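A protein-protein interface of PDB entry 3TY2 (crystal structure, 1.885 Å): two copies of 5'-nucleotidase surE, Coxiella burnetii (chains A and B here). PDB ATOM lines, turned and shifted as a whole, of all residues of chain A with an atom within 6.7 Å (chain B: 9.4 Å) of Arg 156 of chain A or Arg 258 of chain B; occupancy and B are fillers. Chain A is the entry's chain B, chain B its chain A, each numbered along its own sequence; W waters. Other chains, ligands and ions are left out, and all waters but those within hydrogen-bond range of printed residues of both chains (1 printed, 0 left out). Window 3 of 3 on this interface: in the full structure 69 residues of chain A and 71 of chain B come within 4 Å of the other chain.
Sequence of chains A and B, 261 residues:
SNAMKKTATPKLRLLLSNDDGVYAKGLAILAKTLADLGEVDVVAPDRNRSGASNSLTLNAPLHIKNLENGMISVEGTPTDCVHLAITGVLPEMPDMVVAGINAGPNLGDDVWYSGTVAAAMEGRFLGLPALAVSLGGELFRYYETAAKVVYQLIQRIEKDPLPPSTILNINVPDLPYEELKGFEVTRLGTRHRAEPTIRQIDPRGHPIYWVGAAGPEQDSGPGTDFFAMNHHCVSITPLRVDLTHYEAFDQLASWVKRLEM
The guanidinium group (NH1) of Arg 258 of chain B sits at hydrogen-bond distance from the side-chain hydroxyl (OG) of Ser 254 of chain B, 3.0 Å away. The guanidinium group of Arg 156 of chain A is in salt-bridge range of the side-chain carboxylate of Asp 160 of chain A (3.4 Å).
No position is printed for both chains.
Water W1 lies within hydrogen-bond range of the backbone carbonyl oxygen of Trp 255 of chain B (2.7 Å), the side-chain carboxylate of Asp 160 of chain A (2.8 Å), the guanidinium group of Arg 156 of chain A (2.8 Å) and the backbone NH of Leu 259 of chain B (3.4 Å).
Printed residues of chain B within 4 Å of Gln 152 of chain A: Leu 259 (3.6 Å). Printed residues of chain B within 4 Å of Leu 153 of chain A: Trp 255 (3.8 Å) and Leu 259 (3.7 Å). Arg 156 of chain A touches just these residues of chain B: Trp 255 (3.5 Å), Arg 258 (3.97 Å) and Leu 259 (3.4 Å). Of the printed residues of chain B, Ile 157 of chain A touches Trp 255 (3.7 Å). Glu 158 of chain A touches none of the printed residues of chain B. No residue of chain B comes within 4 Å of Lys 159 of chain A. Of the printed residues of chain A, Trp 255 of chain B touches Leu 153 (3.8 Å), Arg 156 (3.5 Å), Ile 157 (3.7 Å), Asp 160 (2.6 Å) and Leu 162 (3.5 Å). Lys 257 of chain B touches none of the printed residues of chain A. Arg 258 of chain B touches just these residues of chain A: Arg 156 (3.97 Å) and Asp 160 (2.6 Å). Printed residues of chain A within 4 Å of Leu 259 of chain B: Gln 152 (3.6 Å), Leu 153 (3.7 Å) and Arg 156 (3.4 Å). The nearest residue of chain B that does not touch Arg 156 of chain A is Met 261 of chain B (5.8 Å). The nearest printed residue of chain B that does not touch Gln 152 of chain A is Trp 255 of chain B (5.8 Å).
The backbone carbonyl oxygen (O) of Asp 160 of chain A sits at hydrogen-bond distance from the indole nitrogen (NE1) of Trp 255 of chain B (2.6 Å). NE of Arg 258 of chain B is in salt-bridge range of OD2 of Asp 160 of chain A, at 2.6 Å.
Hydrophobic or aromatic side chains of chain A within 4 Å of the printed part of chain B: Leu 153, Ile 157 and Leu 162. Of the 12 printed residues of chain B, 3 touch a printed residue of chain A. Printed residues of chain B that touch a printed residue of chain A: Trp 255, Arg 258 and Leu 259. Hydrophobic or aromatic side chains of chain B that line the printed part of chain A: Trp 255 and Leu 259. Among the printed residues, Asp or Glu carboxylates within 4 Å of a Lys or Arg side-chain nitrogen of the other chain: Asp 160 of chain A with Arg 258 of chain B (2.6 Å).
CD1 of Leu 259 of chain B touches O of Gln 152 of chain A (3.6 Å). CD2 of Leu 153 of chain A touches CZ3 of Trp 255 of chain B, 3.8 Å away. CD2 of Leu 153 of chain A touches CD2 of Leu 259 of chain B, at 3.7 Å. CZ2 of Trp 255 of chain B touches CG of Arg 156 of chain A, at 3.5 Å. Arg 156 of chain A touches Arg 258 of chain B. CD1 of Leu 259 of chain B touches CB of Arg 156 of chain A, 3.4 Å away. CG1 of Ile 157 of chain A touches CZ2 of Trp 255 of chain B, 3.7 Å away. Leu 162 of chain A touches Trp 255 of chain B.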
ATOM      1  N   TYR A 151      17.126 -13.664 -10.375  1.00  0.00           N
ATOM      2  CA  TYR A 151      16.417 -13.997  -9.149  1.00  0.00           C
ATOM      3  C   TYR A 151      16.421 -15.513  -8.945  1.00  0.00           C
ATOM      4  O   TYR A 151      16.696 -16.006  -7.855  1.00  0.00           O
ATOM      5  CB  TYR A 151      14.986 -13.461  -9.231  1.00  0.00           C
ATOM      6  CG  TYR A 151      14.191 -13.563  -7.950  1.00  0.00           C
ATOM      7  CD1 TYR A 151      13.465 -14.708  -7.649  1.00  0.00           C
ATOM      8  CD2 TYR A 151      14.149 -12.506  -7.052  1.00  0.00           C
ATOM      9  CE1 TYR A 151      12.728 -14.801  -6.483  1.00  0.00           C
ATOM     10  CE2 TYR A 151      13.417 -12.588  -5.884  1.00  0.00           C
ATOM     11  CZ  TYR A 151      12.707 -13.739  -5.604  1.00  0.00           C
ATOM     12  OH  TYR A 151      11.975 -13.827  -4.442  1.00  0.00           O
ATOM     13  N   GLN A 152      16.147 -16.251 -10.015  1.00  0.00           N
ATOM     14  CA  GLN A 152      16.068 -17.706  -9.942  1.00  0.00           C
ATOM     15  C   GLN A 152      17.426 -18.341  -9.674  1.00  0.00           C
ATOM     16  O   GLN A 152      17.534 -19.273  -8.883  1.00  0.00           O
ATOM     17  CB  GLN A 152      15.459 -18.273 -11.223  1.00  0.00           C
ATOM     18  CG  GLN A 152      13.979 -17.960 -11.371  1.00  0.00           C
ATOM     19  CD  GLN A 152      13.405 -18.417 -12.698  1.00  0.00           C
ATOM     20  OE1 GLN A 152      14.144 -18.755 -13.625  1.00  0.00           O
ATOM     21  NE2 GLN A 152      12.077 -18.433 -12.796  1.00  0.00           N
ATOM     22  N   LEU A 153      18.458 -17.830 -10.337  1.00  0.00           N
ATOM     23  CA  LEU A 153      19.812 -18.332 -10.145  1.00  0.00           C
ATOM     24  C   LEU A 153      20.260 -18.165  -8.697  1.00  0.00           C
ATOM     25  O   LEU A 153      20.881 -19.053  -8.124  1.00  0.00           O
ATOM     26  CB  LEU A 153      20.779 -17.603 -11.087  1.00  0.00           C
ATOM     27  CG  LEU A 153      20.587 -17.970 -12.560  1.00  0.00           C
ATOM     28  CD1 LEU A 153      21.292 -16.979 -13.482  1.00  0.00           C
ATOM     29  CD2 LEU A 153      21.081 -19.378 -12.803  1.00  0.00           C
ATOM     30  N   ILE A 154      19.959 -17.015  -8.108  1.00  0.00           N
ATOM     31  CA  ILE A 154      20.385 -16.763  -6.740  1.00  0.00           C
ATOM     32  C   ILE A 154      19.669 -17.699  -5.758  1.00  0.00           C
ATOM     33  O   ILE A 154      20.311 -18.333  -4.922  1.00  0.00           O
ATOM     34  CB  ILE A 154      20.231 -15.281  -6.349  1.00  0.00           C
ATOM     35  CG1 ILE A 154      21.158 -14.420  -7.216  1.00  0.00           C
ATOM     36  CG2 ILE A 154      20.571 -15.077  -4.879  1.00  0.00           C
ATOM     37  CD1 ILE A 154      20.932 -12.935  -7.088  1.00  0.00           C
ATOM     38  N   GLN A 155      18.351 -17.815  -5.879  1.00  0.00           N
ATOM     39  CA  GLN A 155      17.609 -18.718  -4.998  1.00  0.00           C
ATOM     40  C   GLN A 155      18.207 -20.123  -5.045  1.00  0.00           C
ATOM     41  O   GLN A 155      18.375 -20.775  -4.010  1.00  0.00           O
ATOM     42  CB  GLN A 155      16.114 -18.739  -5.336  1.00  0.00           C
ATOM     43  CG  GLN A 155      15.372 -17.488  -4.880  1.00  0.00           C
ATOM     44  CD  GLN A 155      13.877 -17.717  -4.669  1.00  0.00           C
ATOM     45  OE1 GLN A 155      13.176 -18.216  -5.553  1.00  0.00           O
ATOM     46  NE2 GLN A 155      13.384 -17.345  -3.490  1.00  0.00           N
ATOM     47  N   ARG A 156      18.549 -20.579  -6.244  1.00  0.00           N
ATOM     48  CA  ARG A 156      19.138 -21.905  -6.396  1.00  0.00           C
ATOM     49  C   ARG A 156      20.532 -21.985  -5.770  1.00  0.00           C
ATOM     50  O   ARG A 156      20.856 -22.959  -5.095  1.00  0.00           O
ATOM     51  CB  ARG A 156      19.194 -22.308  -7.868  1.00  0.00           C
ATOM     52  CG  ARG A 156      19.469 -23.773  -8.071  1.00  0.00           C
ATOM     53  CD  ARG A 156      18.387 -24.614  -7.408  1.00  0.00           C
ATOM     54  NE  ARG A 156      18.852 -25.973  -7.164  1.00  0.00           N
ATOM     55  CZ  ARG A 156      18.185 -26.874  -6.455  1.00  0.00           C
ATOM     56  NH1 ARG A 156      17.013 -26.561  -5.918  1.00  0.00           N
ATOM     57  NH2 ARG A 156      18.692 -28.088  -6.286  1.00  0.00           N
ATOM     58  N   ILE A 157      21.349 -20.960  -5.995  1.00  0.00           N
ATOM     59  CA  ILE A 157      22.696 -20.906  -5.431  1.00  0.00           C
ATOM     60  C   ILE A 157      22.668 -21.077  -3.912  1.00  0.00           C
ATOM     61  O   ILE A 157      23.571 -21.671  -3.325  1.00  0.00           O
ATOM     62  CB  ILE A 157      23.419 -19.584  -5.799  1.00  0.00           C
ATOM     63  CG1 ILE A 157      23.781 -19.569  -7.287  1.00  0.00           C
ATOM     64  CG2 ILE A 157      24.680 -19.410  -4.968  1.00  0.00           C
ATOM     65  CD1 ILE A 157      24.192 -18.194  -7.812  1.00  0.00           C
ATOM     66  N   GLU A 158      21.623 -20.556  -3.280  1.00  0.00           N
ATOM     67  CA  GLU A 158      21.453 -20.717  -1.841  1.00  0.00           C
ATOM     68  C   GLU A 158      21.193 -22.174  -1.465  1.00  0.00           C
ATOM     69  O   GLU A 158      21.725 -22.668  -0.475  1.00  0.00           O
ATOM     70  CB  GLU A 158      20.326 -19.818  -1.331  1.00  0.00           C
ATOM     71  CG  GLU A 158      20.668 -18.337  -1.379  1.00  0.00           C
ATOM     72  CD  GLU A 158      19.528 -17.454  -0.908  1.00  0.00           C
ATOM     73  OE1 GLU A 158      18.408 -17.582  -1.445  1.00  0.00           O
ATOM     74  OE2 GLU A 158      19.755 -16.632   0.005  1.00  0.00           O
ATOM     75  N   LYS A 159      20.385 -22.858  -2.269  1.00  0.00           N
ATOM     76  CA  LYS A 159      20.018 -24.250  -2.008  1.00  0.00           C
ATOM     77  C   LYS A 159      21.084 -25.240  -2.462  1.00  0.00           C
ATOM     78  O   LYS A 159      21.168 -26.356  -1.949  1.00  0.00           O
ATOM     79  CB  LYS A 159      18.716 -24.600  -2.735  1.00  0.00           C
ATOM     80  CG  LYS A 159      17.474 -23.879  -2.248  1.00  0.00           C
ATOM     81  CD  LYS A 159      16.251 -24.380  -3.004  1.00  0.00           C
ATOM     82  CE  LYS A 159      15.003 -23.583  -2.657  1.00  0.00           C
ATOM     83  NZ  LYS A 159      13.819 -24.028  -3.449  1.00  0.00           N
ATOM     84  N   ASP A 160      21.894 -24.829  -3.429  1.00  0.00           N
ATOM     85  CA  ASP A 160      22.725 -25.765  -4.172  1.00  0.00           C
ATOM     86  C   ASP A 160      23.995 -25.043  -4.588  1.00  0.00           C
ATOM     87  O   ASP A 160      24.070 -24.486  -5.682  1.00  0.00           O
ATOM     88  CB  ASP A 160      21.944 -26.241  -5.400  1.00  0.00           C
ATOM     89  CG  ASP A 160      22.589 -27.420  -6.100  1.00  0.00           C
ATOM     90  OD1 ASP A 160      23.708 -27.824  -5.725  1.00  0.00           O
ATOM     91  OD2 ASP A 160      21.966 -27.934  -7.051  1.00  0.00           O
ATOM     92  N   PRO A 161      24.991 -25.025  -3.696  1.00  0.00           N
ATOM     93  CA  PRO A 161      26.231 -24.261  -3.877  1.00  0.00           C
ATOM     94  C   PRO A 161      27.039 -24.653  -5.111  1.00  0.00           C
ATOM     95  O   PRO A 161      27.098 -25.826  -5.481  1.00  0.00           O
ATOM     96  CB  PRO A 161      27.022 -24.587  -2.607  1.00  0.00           C
ATOM     97  CG  PRO A 161      25.979 -24.918  -1.597  1.00  0.00           C
ATOM     98  CD  PRO A 161      24.926 -25.655  -2.367  1.00  0.00           C
ATOM     99  N   LEU A 162      27.659 -23.657  -5.738  1.00  0.00           N
ATOM    100  CA  LEU A 162      28.608 -23.886  -6.817  1.00  0.00           C
ATOM    101  C   LEU A 162      30.017 -23.794  -6.251  1.00  0.00           C
ATOM    102  O   LEU A 162      30.205 -23.260  -5.159  1.00  0.00           O
ATOM    103  CB  LEU A 162      28.419 -22.835  -7.910  1.00  0.00           C
ATOM    104  CG  LEU A 162      27.063 -22.877  -8.607  1.00  0.00           C
ATOM    105  CD1 LEU A 162      26.826 -21.607  -9.390  1.00  0.00           C
ATOM    106  CD2 LEU A 162      26.988 -24.109  -9.498  1.00  0.00           C
ATOM    107  N   ASP B 250      30.620 -29.678 -17.075  1.00  0.00           N
ATOM    108  CA  ASP B 250      29.782 -30.810 -16.702  1.00  0.00           C
ATOM    109  C   ASP B 250      29.047 -30.535 -15.403  1.00  0.00           C
ATOM    110  O   ASP B 250      27.835 -30.727 -15.317  1.00  0.00           O
ATOM    111  CB  ASP B 250      30.614 -32.088 -16.594  1.00  0.00           C
ATOM    112  CG  ASP B 250      31.230 -32.489 -17.918  1.00  0.00           C
ATOM    113  OD1 ASP B 250      32.295 -33.144 -17.904  1.00  0.00           O
ATOM    114  OD2 ASP B 250      30.652 -32.143 -18.972  1.00  0.00           O
ATOM    115  N   GLN B 251      29.779 -30.061 -14.399  1.00  0.00           N
ATOM    116  CA  GLN B 251      29.177 -29.775 -13.103  1.00  0.00           C
ATOM    117  C   GLN B 251      28.146 -28.654 -13.208  1.00  0.00           C
ATOM    118  O   GLN B 251      27.068 -28.719 -12.613  1.00  0.00           O
ATOM    119  CB  GLN B 251      30.254 -29.421 -12.081  1.00  0.00           C
ATOM    120  CG  GLN B 251      29.716 -29.113 -10.696  1.00  0.00           C
ATOM    121  CD  GLN B 251      30.808 -29.070  -9.647  1.00  0.00           C
ATOM    122  OE1 GLN B 251      31.974 -29.350  -9.936  1.00  0.00           O
ATOM    123  NE2 GLN B 251      30.438 -28.720  -8.418  1.00  0.00           N
ATOM    124  N   LEU B 252      28.476 -27.617 -13.968  1.00  0.00           N
ATOM    125  CA  LEU B 252      27.550 -26.506 -14.138  1.00  0.00           C
ATOM    126  C   LEU B 252      26.293 -26.926 -14.906  1.00  0.00           C
ATOM    127  O   LEU B 252      25.182 -26.540 -14.551  1.00  0.00           O
ATOM    128  CB  LEU B 252      28.237 -25.339 -14.842  1.00  0.00           C
ATOM    129  CG  LEU B 252      27.380 -24.084 -14.985  1.00  0.00           C
ATOM    130  CD1 LEU B 252      27.019 -23.522 -13.615  1.00  0.00           C
ATOM    131  CD2 LEU B 252      28.117 -23.041 -15.829  1.00  0.00           C
ATOM    132  N   ALA B 253      26.479 -27.714 -15.957  1.00  0.00           N
ATOM    133  CA  ALA B 253      25.361 -28.202 -16.757  1.00  0.00           C
ATOM    134  C   ALA B 253      24.380 -28.998 -15.899  1.00  0.00           C
ATOM    135  O   ALA B 253      23.158 -28.869 -16.040  1.00  0.00           O
ATOM    136  CB  ALA B 253      25.872 -29.051 -17.912  1.00  0.00           C
ATOM    137  N   SER B 254      24.927 -29.819 -15.009  1.00  0.00           N
ATOM    138  CA  SER B 254      24.114 -30.626 -14.113  1.00  0.00           C
ATOM    139  C   SER B 254      23.343 -29.736 -13.144  1.00  0.00           C
ATOM    140  O   SER B 254      22.186 -30.000 -12.828  1.00  0.00           O
ATOM    141  CB  SER B 254      24.998 -31.606 -13.338  1.00  0.00           C
ATOM    142  OG  SER B 254      24.254 -32.265 -12.332  1.00  0.00           O
ATOM    143  N   TRP B 255      23.995 -28.672 -12.688  1.00  0.00           N
ATOM    144  CA  TRP B 255      23.407 -27.753 -11.721  1.00  0.00           C
ATOM    145  C   TRP B 255      22.291 -26.935 -12.369  1.00  0.00           C
ATOM    146  O   TRP B 255      21.280 -26.625 -11.737  1.00  0.00           O
ATOM    147  CB  TRP B 255      24.501 -26.840 -11.169  1.00  0.00           C
ATOM    148  CG  TRP B 255      24.059 -25.862 -10.143  1.00  0.00           C
ATOM    149  CD1 TRP B 255      24.132 -26.003  -8.789  1.00  0.00           C
ATOM    150  CD2 TRP B 255      23.513 -24.563 -10.383  1.00  0.00           C
ATOM    151  NE1 TRP B 255      23.648 -24.878  -8.171  1.00  0.00           N
ATOM    152  CE2 TRP B 255      23.263 -23.977  -9.129  1.00  0.00           C
ATOM    153  CE3 TRP B 255      23.203 -23.843 -11.540  1.00  0.00           C
ATOM    154  CZ2 TRP B 255      22.718 -22.706  -8.998  1.00  0.00           C
ATOM    155  CZ3 TRP B 255      22.668 -22.583 -11.409  1.00  0.00           C
ATOM    156  CH2 TRP B 255      22.429 -22.025 -10.147  1.00  0.00           C
ATOM    157  N   VAL B 256      22.473 -26.589 -13.637  1.00  0.00           N
ATOM    158  CA  VAL B 256      21.456 -25.830 -14.351  1.00  0.00           C
ATOM    159  C   VAL B 256      20.202 -26.685 -14.566  1.00  0.00           C
ATOM    160  O   VAL B 256      19.087 -26.162 -14.612  1.00  0.00           O
ATOM    161  CB  VAL B 256      21.980 -25.276 -15.693  1.00  0.00           C
ATOM    162  CG1 VAL B 256      20.839 -24.686 -16.509  1.00  0.00           C
ATOM    163  CG2 VAL B 256      23.053 -24.213 -15.449  1.00  0.00           C
ATOM    164  N   LYS B 257      20.382 -28.000 -14.679  1.00  0.00           N
ATOM    165  CA  LYS B 257      19.235 -28.890 -14.830  1.00  0.00           C
ATOM    166  C   LYS B 257      18.417 -28.935 -13.547  1.00  0.00           C
ATOM    167  O   LYS B 257      17.186 -28.928 -13.585  1.00  0.00           O
ATOM    168  CB  LYS B 257      19.676 -30.295 -15.238  1.00  0.00           C
ATOM    169  CG  LYS B 257      20.293 -30.381 -16.620  1.00  0.00           C
ATOM    170  CD  LYS B 257      20.811 -31.788 -16.873  1.00  0.00           C
ATOM    171  CE  LYS B 257      21.696 -31.857 -18.110  1.00  0.00           C
ATOM    172  NZ  LYS B 257      22.341 -33.202 -18.218  1.00  0.00           N
ATOM    173  N   ARG B 258      19.107 -28.980 -12.411  1.00  0.00           N
ATOM    174  CA  ARG B 258      18.444 -28.968 -11.115  1.00  0.00           C
ATOM    175  C   ARG B 258      17.755 -27.630 -10.871  1.00  0.00           C
ATOM    176  O   ARG B 258      16.732 -27.561 -10.190  1.00  0.00           O
ATOM    177  CB  ARG B 258      19.447 -29.267 -10.006  1.00  0.00           C
ATOM    178  CG  ARG B 258      20.141 -30.597 -10.187  1.00  0.00           C
ATOM    179  CD  ARG B 258      20.815 -31.045  -8.908  1.00  0.00           C
ATOM    180  NE  ARG B 258      21.855 -30.119  -8.473  1.00  0.00           N
ATOM    181  CZ  ARG B 258      23.123 -30.189  -8.858  1.00  0.00           C
ATOM    182  NH1 ARG B 258      23.509 -31.135  -9.699  1.00  0.00           N
ATOM    183  NH2 ARG B 258      24.005 -29.310  -8.407  1.00  0.00           N
ATOM    184  N   LEU B 259      18.324 -26.570 -11.431  1.00  0.00           N
ATOM    185  CA  LEU B 259      17.682 -25.264 -11.422  1.00  0.00           C
ATOM    186  C   LEU B 259      16.319 -25.366 -12.094  1.00  0.00           C
ATOM    187  O   LEU B 259      15.322 -24.847 -11.592  1.00  0.00           O
ATOM    188  CB  LEU B 259      18.544 -24.254 -12.178  1.00  0.00           C
ATOM    189  CG  LEU B 259      17.942 -22.862 -12.376  1.00  0.00           C
ATOM    190  CD1 LEU B 259      17.973 -22.081 -11.074  1.00  0.00           C
ATOM    191  CD2 LEU B 259      18.688 -22.109 -13.465  1.00  0.00           C
ATOM    192  N   GLU B 260      16.293 -26.053 -13.234  1.00  0.00           N
ATOM    193  CA  GLU B 260      15.093 -26.160 -14.060  1.00  0.00           C
ATOM    194  C   GLU B 260      14.055 -27.120 -13.486  1.00  0.00           C
ATOM    195  O   GLU B 260      12.945 -27.222 -14.008  1.00  0.00           O
ATOM    196  CB  GLU B 260      15.462 -26.602 -15.478  1.00  0.00           C
ATOM    197  CG  GLU B 260      16.400 -25.659 -16.219  1.00  0.00           C
ATOM    198  CD  GLU B 260      16.756 -26.175 -17.601  1.00  0.00           C
ATOM    199  OE1 GLU B 260      16.365 -27.314 -17.926  1.00  0.00           O
ATOM    200  OE2 GLU B 260      17.420 -25.446 -18.367  1.00  0.00           O
ATOM    201  N   MET B 261      14.411 -27.828 -12.419  1.00  0.00           N
ATOM    202  CA  MET B 261      13.497 -28.797 -11.821  1.00  0.00           C
ATOM    203  C   MET B 261      12.265 -28.122 -11.228  1.00  0.00           C
ATOM    204  O   MET B 261      12.161 -26.896 -11.195  1.00  0.00           O
ATOM    205  OXT MET B 261      11.339 -28.788 -10.774  1.00  0.00           O
ATOM    206  CB  MET B 261      14.211 -29.643 -10.761  1.00  0.00           C
ATOM    207  CG  MET B 261      15.341 -30.492 -11.319  1.00  0.00           C
ATOM    208  SD  MET B 261      16.104 -31.744 -10.031  1.00  0.00           S
ATOM    209  CE  MET B 261      14.490 -32.745  -9.606  1.00  0.00           C
HETATM  210  O   HOH W   1      20.846 -26.452  -9.091  1.00  0.00           O
